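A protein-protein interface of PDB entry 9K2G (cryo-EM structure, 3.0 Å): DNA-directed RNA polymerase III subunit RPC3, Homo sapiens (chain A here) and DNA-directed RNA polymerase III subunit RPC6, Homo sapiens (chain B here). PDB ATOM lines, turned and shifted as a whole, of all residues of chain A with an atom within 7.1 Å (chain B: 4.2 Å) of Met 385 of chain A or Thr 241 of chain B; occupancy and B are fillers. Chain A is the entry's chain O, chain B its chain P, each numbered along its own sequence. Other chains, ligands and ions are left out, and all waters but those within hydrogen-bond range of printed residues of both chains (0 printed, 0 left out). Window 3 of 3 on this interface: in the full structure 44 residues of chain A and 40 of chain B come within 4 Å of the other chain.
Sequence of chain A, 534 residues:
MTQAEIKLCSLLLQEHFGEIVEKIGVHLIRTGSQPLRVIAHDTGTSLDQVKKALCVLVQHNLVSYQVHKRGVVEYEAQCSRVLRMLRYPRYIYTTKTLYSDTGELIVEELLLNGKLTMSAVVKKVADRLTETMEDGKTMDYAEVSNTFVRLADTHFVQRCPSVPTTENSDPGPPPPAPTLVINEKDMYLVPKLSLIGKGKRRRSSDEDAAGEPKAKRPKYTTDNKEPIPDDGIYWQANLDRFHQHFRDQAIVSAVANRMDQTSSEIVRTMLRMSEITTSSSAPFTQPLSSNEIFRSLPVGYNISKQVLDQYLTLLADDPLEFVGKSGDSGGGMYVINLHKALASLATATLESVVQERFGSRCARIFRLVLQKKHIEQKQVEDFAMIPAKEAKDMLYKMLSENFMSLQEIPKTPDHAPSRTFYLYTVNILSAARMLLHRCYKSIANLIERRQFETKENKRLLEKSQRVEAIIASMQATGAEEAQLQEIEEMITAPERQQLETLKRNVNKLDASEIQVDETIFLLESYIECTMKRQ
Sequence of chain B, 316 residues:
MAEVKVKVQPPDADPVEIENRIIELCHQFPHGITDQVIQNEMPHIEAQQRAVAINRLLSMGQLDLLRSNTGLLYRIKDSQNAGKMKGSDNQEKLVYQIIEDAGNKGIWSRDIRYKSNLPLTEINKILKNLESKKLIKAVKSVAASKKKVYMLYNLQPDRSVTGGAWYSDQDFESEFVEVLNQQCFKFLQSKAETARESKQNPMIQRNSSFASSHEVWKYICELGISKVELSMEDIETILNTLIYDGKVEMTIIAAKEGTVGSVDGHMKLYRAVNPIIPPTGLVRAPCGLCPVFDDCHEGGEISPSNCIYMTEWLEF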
ATOM      1  N   ARG A 361      24.576 -24.069   6.998  1.00  0.00           N
ATOM      2  CA  ARG A 361      23.592 -23.903   8.065  1.00  0.00           C
ATOM      3  C   ARG A 361      22.169 -23.967   7.518  1.00  0.00           C
ATOM      4  O   ARG A 361      21.291 -24.618   8.106  1.00  0.00           O
ATOM      5  CB  ARG A 361      23.838 -22.582   8.799  1.00  0.00           C
ATOM      6  CG  ARG A 361      25.294 -22.363   9.226  1.00  0.00           C
ATOM      7  CD  ARG A 361      25.457 -21.028   9.939  1.00  0.00           C
ATOM      8  NE  ARG A 361      24.669 -20.973  11.166  1.00  0.00           N
ATOM      9  CZ  ARG A 361      25.131 -21.307  12.366  1.00  0.00           C
ATOM     10  NH1 ARG A 361      26.372 -21.726  12.536  1.00  0.00           N
ATOM     11  NH2 ARG A 361      24.324 -21.219  13.418  1.00  0.00           N
ATOM     12  N   ARG A 364      21.389 -27.437   6.831  1.00  0.00           N
ATOM     13  CA  ARG A 364      21.038 -28.113   8.074  1.00  0.00           C
ATOM     14  C   ARG A 364      19.572 -27.894   8.415  1.00  0.00           C
ATOM     15  O   ARG A 364      18.852 -28.840   8.763  1.00  0.00           O
ATOM     16  CB  ARG A 364      21.941 -27.612   9.204  1.00  0.00           C
ATOM     17  CG  ARG A 364      21.542 -28.091  10.589  1.00  0.00           C
ATOM     18  CD  ARG A 364      22.324 -27.331  11.649  1.00  0.00           C
ATOM     19  NE  ARG A 364      23.747 -27.302  11.346  1.00  0.00           N
ATOM     20  CZ  ARG A 364      24.632 -26.539  11.966  1.00  0.00           C
ATOM     21  NH1 ARG A 364      24.272 -25.712  12.936  1.00  0.00           N
ATOM     22  NH2 ARG A 364      25.909 -26.595  11.604  1.00  0.00           N
ATOM     23  N   LEU A 368      16.671 -30.763   8.476  1.00  0.00           N
ATOM     24  CA  LEU A 368      15.870 -30.914   9.689  1.00  0.00           C
ATOM     25  C   LEU A 368      14.382 -30.862   9.378  1.00  0.00           C
ATOM     26  O   LEU A 368      13.612 -31.732   9.814  1.00  0.00           O
ATOM     27  CB  LEU A 368      16.247 -29.830  10.697  1.00  0.00           C
ATOM     28  CG  LEU A 368      15.232 -29.554  11.810  1.00  0.00           C
ATOM     29  CD1 LEU A 368      15.052 -30.759  12.726  1.00  0.00           C
ATOM     30  CD2 LEU A 368      15.633 -28.323  12.609  1.00  0.00           C
ATOM     31  N   GLN A 379      10.889 -25.099  17.639  1.00  0.00           N
ATOM     32  CA  GLN A 379      11.429 -26.452  17.540  1.00  0.00           C
ATOM     33  C   GLN A 379      12.629 -26.497  16.603  1.00  0.00           C
ATOM     34  O   GLN A 379      13.598 -27.222  16.861  1.00  0.00           O
ATOM     35  CB  GLN A 379      10.336 -27.412  17.082  1.00  0.00           C
ATOM     36  CG  GLN A 379       9.036 -27.271  17.860  1.00  0.00           C
ATOM     37  CD  GLN A 379       7.870 -27.943  17.170  1.00  0.00           C
ATOM     38  OE1 GLN A 379       8.052 -28.810  16.312  1.00  0.00           O
ATOM     39  NE2 GLN A 379       6.656 -27.542  17.533  1.00  0.00           N
ATOM     40  N   VAL A 380      12.585 -25.732  15.504  1.00  0.00           N
ATOM     41  CA  VAL A 380      13.722 -25.668  14.590  1.00  0.00           C
ATOM     42  C   VAL A 380      14.948 -25.122  15.311  1.00  0.00           C
ATOM     43  O   VAL A 380      16.053 -25.665  15.196  1.00  0.00           O
ATOM     44  CB  VAL A 380      13.373 -24.818  13.355  1.00  0.00           C
ATOM     45  CG1 VAL A 380      14.633 -24.465  12.579  1.00  0.00           C
ATOM     46  CG2 VAL A 380      12.392 -25.552  12.461  1.00  0.00           C
ATOM     47  N   GLU A 381      14.768 -24.034  16.065  1.00  0.00           N
ATOM     48  CA  GLU A 381      15.885 -23.455  16.805  1.00  0.00           C
ATOM     49  C   GLU A 381      16.409 -24.418  17.861  1.00  0.00           C
ATOM     50  O   GLU A 381      17.624 -24.518  18.071  1.00  0.00           O
ATOM     51  CB  GLU A 381      15.461 -22.135  17.446  1.00  0.00           C
ATOM     52  CG  GLU A 381      15.066 -21.059  16.443  1.00  0.00           C
ATOM     53  CD  GLU A 381      14.662 -19.762  17.109  1.00  0.00           C
ATOM     54  OE1 GLU A 381      14.483 -19.755  18.347  1.00  0.00           O
ATOM     55  OE2 GLU A 381      14.522 -18.746  16.398  1.00  0.00           O
ATOM     56  N   ASP A 382      15.511 -25.135  18.537  1.00  0.00           N
ATOM     57  CA  ASP A 382      15.936 -26.076  19.566  1.00  0.00           C
ATOM     58  C   ASP A 382      16.704 -27.252  18.974  1.00  0.00           C
ATOM     59  O   ASP A 382      17.667 -27.735  19.579  1.00  0.00           O
ATOM     60  CB  ASP A 382      14.719 -26.572  20.350  1.00  0.00           C
ATOM     61  CG  ASP A 382      14.037 -25.465  21.129  1.00  0.00           C
ATOM     62  OD1 ASP A 382      14.585 -24.345  21.171  1.00  0.00           O
ATOM     63  OD2 ASP A 382      12.950 -25.717  21.690  1.00  0.00           O
ATOM     64  N   PHE A 383      16.291 -27.737  17.804  1.00  0.00           N
ATOM     65  CA  PHE A 383      16.904 -28.927  17.219  1.00  0.00           C
ATOM     66  C   PHE A 383      18.131 -28.626  16.367  1.00  0.00           C
ATOM     67  O   PHE A 383      18.951 -29.527  16.152  1.00  0.00           O
ATOM     68  CB  PHE A 383      15.885 -29.692  16.370  1.00  0.00           C
ATOM     69  CG  PHE A 383      14.869 -30.455  17.175  1.00  0.00           C
ATOM     70  CD1 PHE A 383      14.893 -30.425  18.561  1.00  0.00           C
ATOM     71  CD2 PHE A 383      13.899 -31.216  16.544  1.00  0.00           C
ATOM     72  CE1 PHE A 383      13.959 -31.127  19.301  1.00  0.00           C
ATOM     73  CE2 PHE A 383      12.968 -31.923  17.278  1.00  0.00           C
ATOM     74  CZ  PHE A 383      12.999 -31.878  18.654  1.00  0.00           C
ATOM     75  N   ALA A 384      18.281 -27.398  15.871  1.00  0.00           N
ATOM     76  CA  ALA A 384      19.381 -27.064  14.978  1.00  0.00           C
ATOM     77  C   ALA A 384      20.553 -26.390  15.679  1.00  0.00           C
ATOM     78  O   ALA A 384      21.640 -26.320  15.096  1.00  0.00           O
ATOM     79  CB  ALA A 384      18.882 -26.155  13.846  1.00  0.00           C
ATOM     80  N   MET A 385      20.364 -25.909  16.911  1.00  0.00           N
ATOM     81  CA  MET A 385      21.382 -25.142  17.632  1.00  0.00           C
ATOM     82  C   MET A 385      21.880 -23.969  16.793  1.00  0.00           C
ATOM     83  O   MET A 385      23.075 -23.670  16.744  1.00  0.00           O
ATOM     84  CB  MET A 385      22.546 -26.033  18.076  1.00  0.00           C
ATOM     85  CG  MET A 385      22.134 -27.212  18.943  1.00  0.00           C
ATOM     86  SD  MET A 385      20.661 -26.902  19.946  1.00  0.00           S
ATOM     87  CE  MET A 385      21.262 -25.706  21.143  1.00  0.00           C
ATOM     88  N   ILE A 386      20.955 -23.308  16.119  1.00  0.00           N
ATOM     89  CA  ILE A 386      21.224 -22.116  15.323  1.00  0.00           C
ATOM     90  C   ILE A 386      20.564 -20.933  16.022  1.00  0.00           C
ATOM     91  O   ILE A 386      19.369 -20.996  16.317  1.00  0.00           O
ATOM     92  CB  ILE A 386      20.712 -22.258  13.882  1.00  0.00           C
ATOM     93  CG1 ILE A 386      21.501 -23.350  13.154  1.00  0.00           C
ATOM     94  CG2 ILE A 386      20.809 -20.935  13.135  1.00  0.00           C
ATOM     95  CD1 ILE A 386      21.054 -23.590  11.737  1.00  0.00           C
ATOM     96  N   PRO A 387      21.300 -19.857  16.310  1.00  0.00           N
ATOM     97  CA  PRO A 387      20.717 -18.756  17.090  1.00  0.00           C
ATOM     98  C   PRO A 387      19.549 -18.099  16.363  1.00  0.00           C
ATOM     99  O   PRO A 387      19.482 -18.089  15.134  1.00  0.00           O
ATOM    100  CB  PRO A 387      21.888 -17.781  17.260  1.00  0.00           C
ATOM    101  CG  PRO A 387      22.807 -18.097  16.119  1.00  0.00           C
ATOM    102  CD  PRO A 387      22.686 -19.577  15.910  1.00  0.00           C
ATOM    103  N   TRP B 166      24.858 -24.279  26.438  1.00  0.00           N
ATOM    104  CA  TRP B 166      25.233 -23.396  25.344  1.00  0.00           C
ATOM    105  C   TRP B 166      25.149 -21.928  25.736  1.00  0.00           C
ATOM    106  O   TRP B 166      26.021 -21.136  25.358  1.00  0.00           O
ATOM    107  CB  TRP B 166      24.338 -23.644  24.129  1.00  0.00           C
ATOM    108  CG  TRP B 166      24.243 -25.084  23.730  1.00  0.00           C
ATOM    109  CD1 TRP B 166      25.146 -25.789  22.986  1.00  0.00           C
ATOM    110  CD2 TRP B 166      23.183 -25.993  24.040  1.00  0.00           C
ATOM    111  NE1 TRP B 166      24.714 -27.082  22.824  1.00  0.00           N
ATOM    112  CE2 TRP B 166      23.510 -27.234  23.459  1.00  0.00           C
ATOM    113  CE3 TRP B 166      21.984 -25.882  24.756  1.00  0.00           C
ATOM    114  CZ2 TRP B 166      22.687 -28.355  23.567  1.00  0.00           C
ATOM    115  CZ3 TRP B 166      21.172 -26.995  24.866  1.00  0.00           C
ATOM    116  CH2 TRP B 166      21.524 -28.216  24.275  1.00  0.00           C
ATOM    117  N   PHE B 172      23.946 -16.974  23.169  1.00  0.00           N
ATOM    118  CA  PHE B 172      24.196 -18.241  22.502  1.00  0.00           C
ATOM    119  C   PHE B 172      25.636 -18.293  22.018  1.00  0.00           C
ATOM    120  O   PHE B 172      26.156 -17.321  21.458  1.00  0.00           O
ATOM    121  CB  PHE B 172      23.232 -18.435  21.332  1.00  0.00           C
ATOM    122  CG  PHE B 172      23.296 -19.798  20.707  1.00  0.00           C
ATOM    123  CD1 PHE B 172      22.508 -20.833  21.191  1.00  0.00           C
ATOM    124  CD2 PHE B 172      24.145 -20.056  19.646  1.00  0.00           C
ATOM    125  CE1 PHE B 172      22.564 -22.092  20.624  1.00  0.00           C
ATOM    126  CE2 PHE B 172      24.204 -21.311  19.072  1.00  0.00           C
ATOM    127  CZ  PHE B 172      23.416 -22.331  19.564  1.00  0.00           C
ATOM    128  N   ASN B 181      30.961 -29.351  16.943  1.00  0.00           N
ATOM    129  CA  ASN B 181      30.687 -30.037  15.685  1.00  0.00           C
ATOM    130  C   ASN B 181      31.973 -30.473  15.007  1.00  0.00           C
ATOM    131  O   ASN B 181      32.079 -31.612  14.532  1.00  0.00           O
ATOM    132  CB  ASN B 181      29.879 -29.130  14.757  1.00  0.00           C
ATOM    133  CG  ASN B 181      28.380 -29.317  14.921  1.00  0.00           C
ATOM    134  OD1 ASN B 181      27.915 -29.859  15.921  1.00  0.00           O
ATOM    135  ND2 ASN B 181      27.615 -28.866  13.928  1.00  0.00           N
ATOM    136  N   THR B 237      22.489 -34.163  21.263  1.00  0.00           N
ATOM    137  CA  THR B 237      21.933 -33.065  20.477  1.00  0.00           C
ATOM    138  C   THR B 237      22.943 -32.535  19.468  1.00  0.00           C
ATOM    139  O   THR B 237      22.580 -32.195  18.333  1.00  0.00           O
ATOM    140  CB  THR B 237      21.462 -31.936  21.399  1.00  0.00           C
ATOM    141  OG1 THR B 237      22.536 -31.544  22.259  1.00  0.00           O
ATOM    142  CG2 THR B 237      20.279 -32.390  22.237  1.00  0.00           C
ATOM    143  N   ILE B 238      24.215 -32.445  19.865  1.00  0.00           N
ATOM    144  CA  ILE B 238      25.249 -32.007  18.930  1.00  0.00           C
ATOM    145  C   ILE B 238      25.345 -32.965  17.750  1.00  0.00           C
ATOM    146  O   ILE B 238      25.426 -32.547  16.584  1.00  0.00           O
ATOM    147  CB  ILE B 238      26.605 -31.866  19.658  1.00  0.00           C
ATOM    148  CG1 ILE B 238      26.511 -30.818  20.770  1.00  0.00           C
ATOM    149  CG2 ILE B 238      27.703 -31.499  18.680  1.00  0.00           C
ATOM    150  CD1 ILE B 238      26.100 -29.444  20.288  1.00  0.00           C
ATOM    151  N   LEU B 239      25.321 -34.272  18.030  1.00  0.00           N
ATOM    152  CA  LEU B 239      25.348 -35.264  16.962  1.00  0.00           C
ATOM    153  C   LEU B 239      24.086 -35.210  16.109  1.00  0.00           C
ATOM    154  O   LEU B 239      24.149 -35.472  14.908  1.00  0.00           O
ATOM    155  CB  LEU B 239      25.542 -36.662  17.543  1.00  0.00           C
ATOM    156  CG  LEU B 239      26.884 -36.928  18.225  1.00  0.00           C
ATOM    157  CD1 LEU B 239      26.967 -38.379  18.660  1.00  0.00           C
ATOM    158  CD2 LEU B 239      28.043 -36.572  17.305  1.00  0.00           C
ATOM    159  N   ASN B 240      22.935 -34.889  16.707  1.00  0.00           N
ATOM    160  CA  ASN B 240      21.721 -34.720  15.919  1.00  0.00           C
ATOM    161  C   ASN B 240      21.850 -33.548  14.954  1.00  0.00           C
ATOM    162  O   ASN B 240      21.420 -33.630  13.797  1.00  0.00           O
ATOM    163  CB  ASN B 240      20.513 -34.524  16.840  1.00  0.00           C
ATOM    164  CG  ASN B 240      19.823 -35.828  17.176  1.00  0.00           C
ATOM    165  OD1 ASN B 240      19.693 -36.709  16.326  1.00  0.00           O
ATOM    166  ND2 ASN B 240      19.373 -35.958  18.420  1.00  0.00           N
ATOM    167  N   THR B 241      22.436 -32.442  15.417  1.00  0.00           N
ATOM    168  CA  THR B 241      22.685 -31.311  14.524  1.00  0.00           C
ATOM    169  C   THR B 241      23.647 -31.704  13.406  1.00  0.00           C
ATOM    170  O   THR B 241      23.470 -31.297  12.250  1.00  0.00           O
ATOM    171  CB  THR B 241      23.238 -30.117  15.302  1.00  0.00           C
ATOM    172  OG1 THR B 241      24.499 -30.466  15.889  1.00  0.00           O
ATOM    173  CG2 THR B 241      22.270 -29.705  16.395  1.00  0.00           C
ATOM    174  N   LEU B 242      24.669 -32.494  13.733  1.00  0.00           N
ATOM    175  CA  LEU B 242      25.579 -32.991  12.705  1.00  0.00           C
ATOM    176  C   LEU B 242      24.847 -33.890  11.708  1.00  0.00           C
ATOM    177  O   LEU B 242      25.161 -33.887  10.515  1.00  0.00           O
ATOM    178  CB  LEU B 242      26.746 -33.727  13.352  1.00  0.00           C
ATOM    179  CG  LEU B 242      27.874 -32.849  13.904  1.00  0.00           C
ATOM    180  CD1 LEU B 242      28.792 -33.655  14.800  1.00  0.00           C
ATOM    181  CD2 LEU B 242      28.655 -32.218  12.762  1.00  0.00           C
ATOM    182  N   ILE B 243      23.883 -34.680  12.192  1.00  0.00           N
ATOM    183  CA  ILE B 243      23.054 -35.490  11.305  1.00  0.00           C
ATOM    184  C   ILE B 243      22.281 -34.594  10.348  1.00  0.00           C
ATOM    185  O   ILE B 243      22.220 -34.843   9.138  1.00  0.00           O
ATOM    186  CB  ILE B 243      22.100 -36.383  12.121  1.00  0.00           C
ATOM    187  CG1 ILE B 243      22.872 -37.459  12.877  1.00  0.00           C
ATOM    188  CG2 ILE B 243      21.051 -37.014  11.216  1.00  0.00           C
ATOM    189  CD1 ILE B 243      22.047 -38.145  13.935  1.00  0.00           C
ATOM    190  N   TYR B 244      21.675 -33.533  10.885  1.00  0.00           N
ATOM    191  CA  TYR B 244      20.944 -32.592  10.044  1.00  0.00           C
ATOM    192  C   TYR B 244      21.860 -31.857   9.080  1.00  0.00           C
ATOM    193  O   TYR B 244      21.375 -31.273   8.106  1.00  0.00           O
ATOM    194  CB  TYR B 244      20.178 -31.601  10.924  1.00  0.00           C
ATOM    195  CG  TYR B 244      19.145 -32.263  11.808  1.00  0.00           C
ATOM    196  CD1 TYR B 244      18.454 -33.385  11.379  1.00  0.00           C
ATOM    197  CD2 TYR B 244      18.877 -31.772  13.082  1.00  0.00           C
ATOM    198  CE1 TYR B 244      17.515 -34.000  12.187  1.00  0.00           C
ATOM    199  CE2 TYR B 244      17.938 -32.381  13.895  1.00  0.00           C
ATOM    200  CZ  TYR B 244      17.261 -33.494  13.443  1.00  0.00           C
ATOM    201  OH  TYR B 244      16.328 -34.103  14.249  1.00  0.00           O
ATOM    202  N   ASP B 245      23.167 -31.876   9.321  1.00  0.00           N
ATOM    203  CA  ASP B 245      24.132 -31.313   8.386  1.00  0.00           C
ATOM    204  C   ASP B 245      24.457 -32.266   7.241  1.00  0.00           C
ATOM    205  O   ASP B 245      25.195 -31.884   6.327  1.00  0.00           O
ATOM    206  CB  ASP B 245      25.416 -30.929   9.127  1.00  0.00           C
ATOM    207  CG  ASP B 245      26.173 -29.810   8.443  1.00  0.00           C
ATOM    208  OD1 ASP B 245      25.693 -29.313   7.402  1.00  0.00           O
ATOM    209  OD2 ASP B 245      27.246 -29.417   8.953  1.00  0.00           O
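Arg 364 of chain A touches Asn 181 of chain B (NH2 to ND2, 3.7 Å). Arg 364 of chain A touches Tyr 244 of chain B. Leu 368 of chain A touches Tyr 244 of chain B. CG2 of Thr 241 of chain B touches O of Phe 383 of chain A, at 3.3 Å. Phe 383 of chain A touches Tyr 244 of chain B (O to CE2, 3.8 Å). Ala 384 of chain A touches Thr 241 of chain B (O to CG2, 3.7 Å). Trp 166 of chain B touches Met 385 of chain A. Phe 172 of chain B touches Met 385 of chain A. Thr 241 of chain B touches Met 385 of chain A. CE2 of Phe 172 of chain B touches CD of Pro 387 of chain A, 3.9 Å away.
The backbone carbonyl oxygen (O) of Ala 384 of chain A sits at hydrogen-bond distance from the guanidinium group (NH1) of Arg 364 of chain A, at 3.5 Å. OG1 of Thr 241 of chain B sits at hydrogen-bond distance from OD1 of Asn 181 of chain B (3.5 Å).
Of the 12 printed residues of chain A, 6 touch a printed residue of chain B. Hydrophobic or aromatic side chains of chain A within 4 Å of the printed part of chain B: Leu 368, Met 385 and Pro 387. Among the printed residues, 10 pairs touch across the chains. Among the printed residues, no Asp or Glu carboxylate lies within 4 Å of a Lys or Arg side-chain nitrogen of the other chain.
Of the printed residues of chain B, Arg 364 of chain A touches Asn 181 (3.7 Å) and Tyr 244 (3.2 Å). Of the printed residues of chain B, Leu 368 of chain A touches Tyr 244 (3.5 Å). Val 380 of chain A touches none of the printed residues of chain B. Printed residues of chain B within 4 Å of Phe 383 of chain A: Thr 241 and Tyr 244. Of chain B, only Trp 166, Phe 172 and Thr 241 come within 4 Å of Met 385 of chain A. Asn 240 of chain B touches none of the printed residues of chain A. Of chain A, only Phe 383, Ala 384 and Met 385 come within 4 Å of Thr 241 of chain B.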
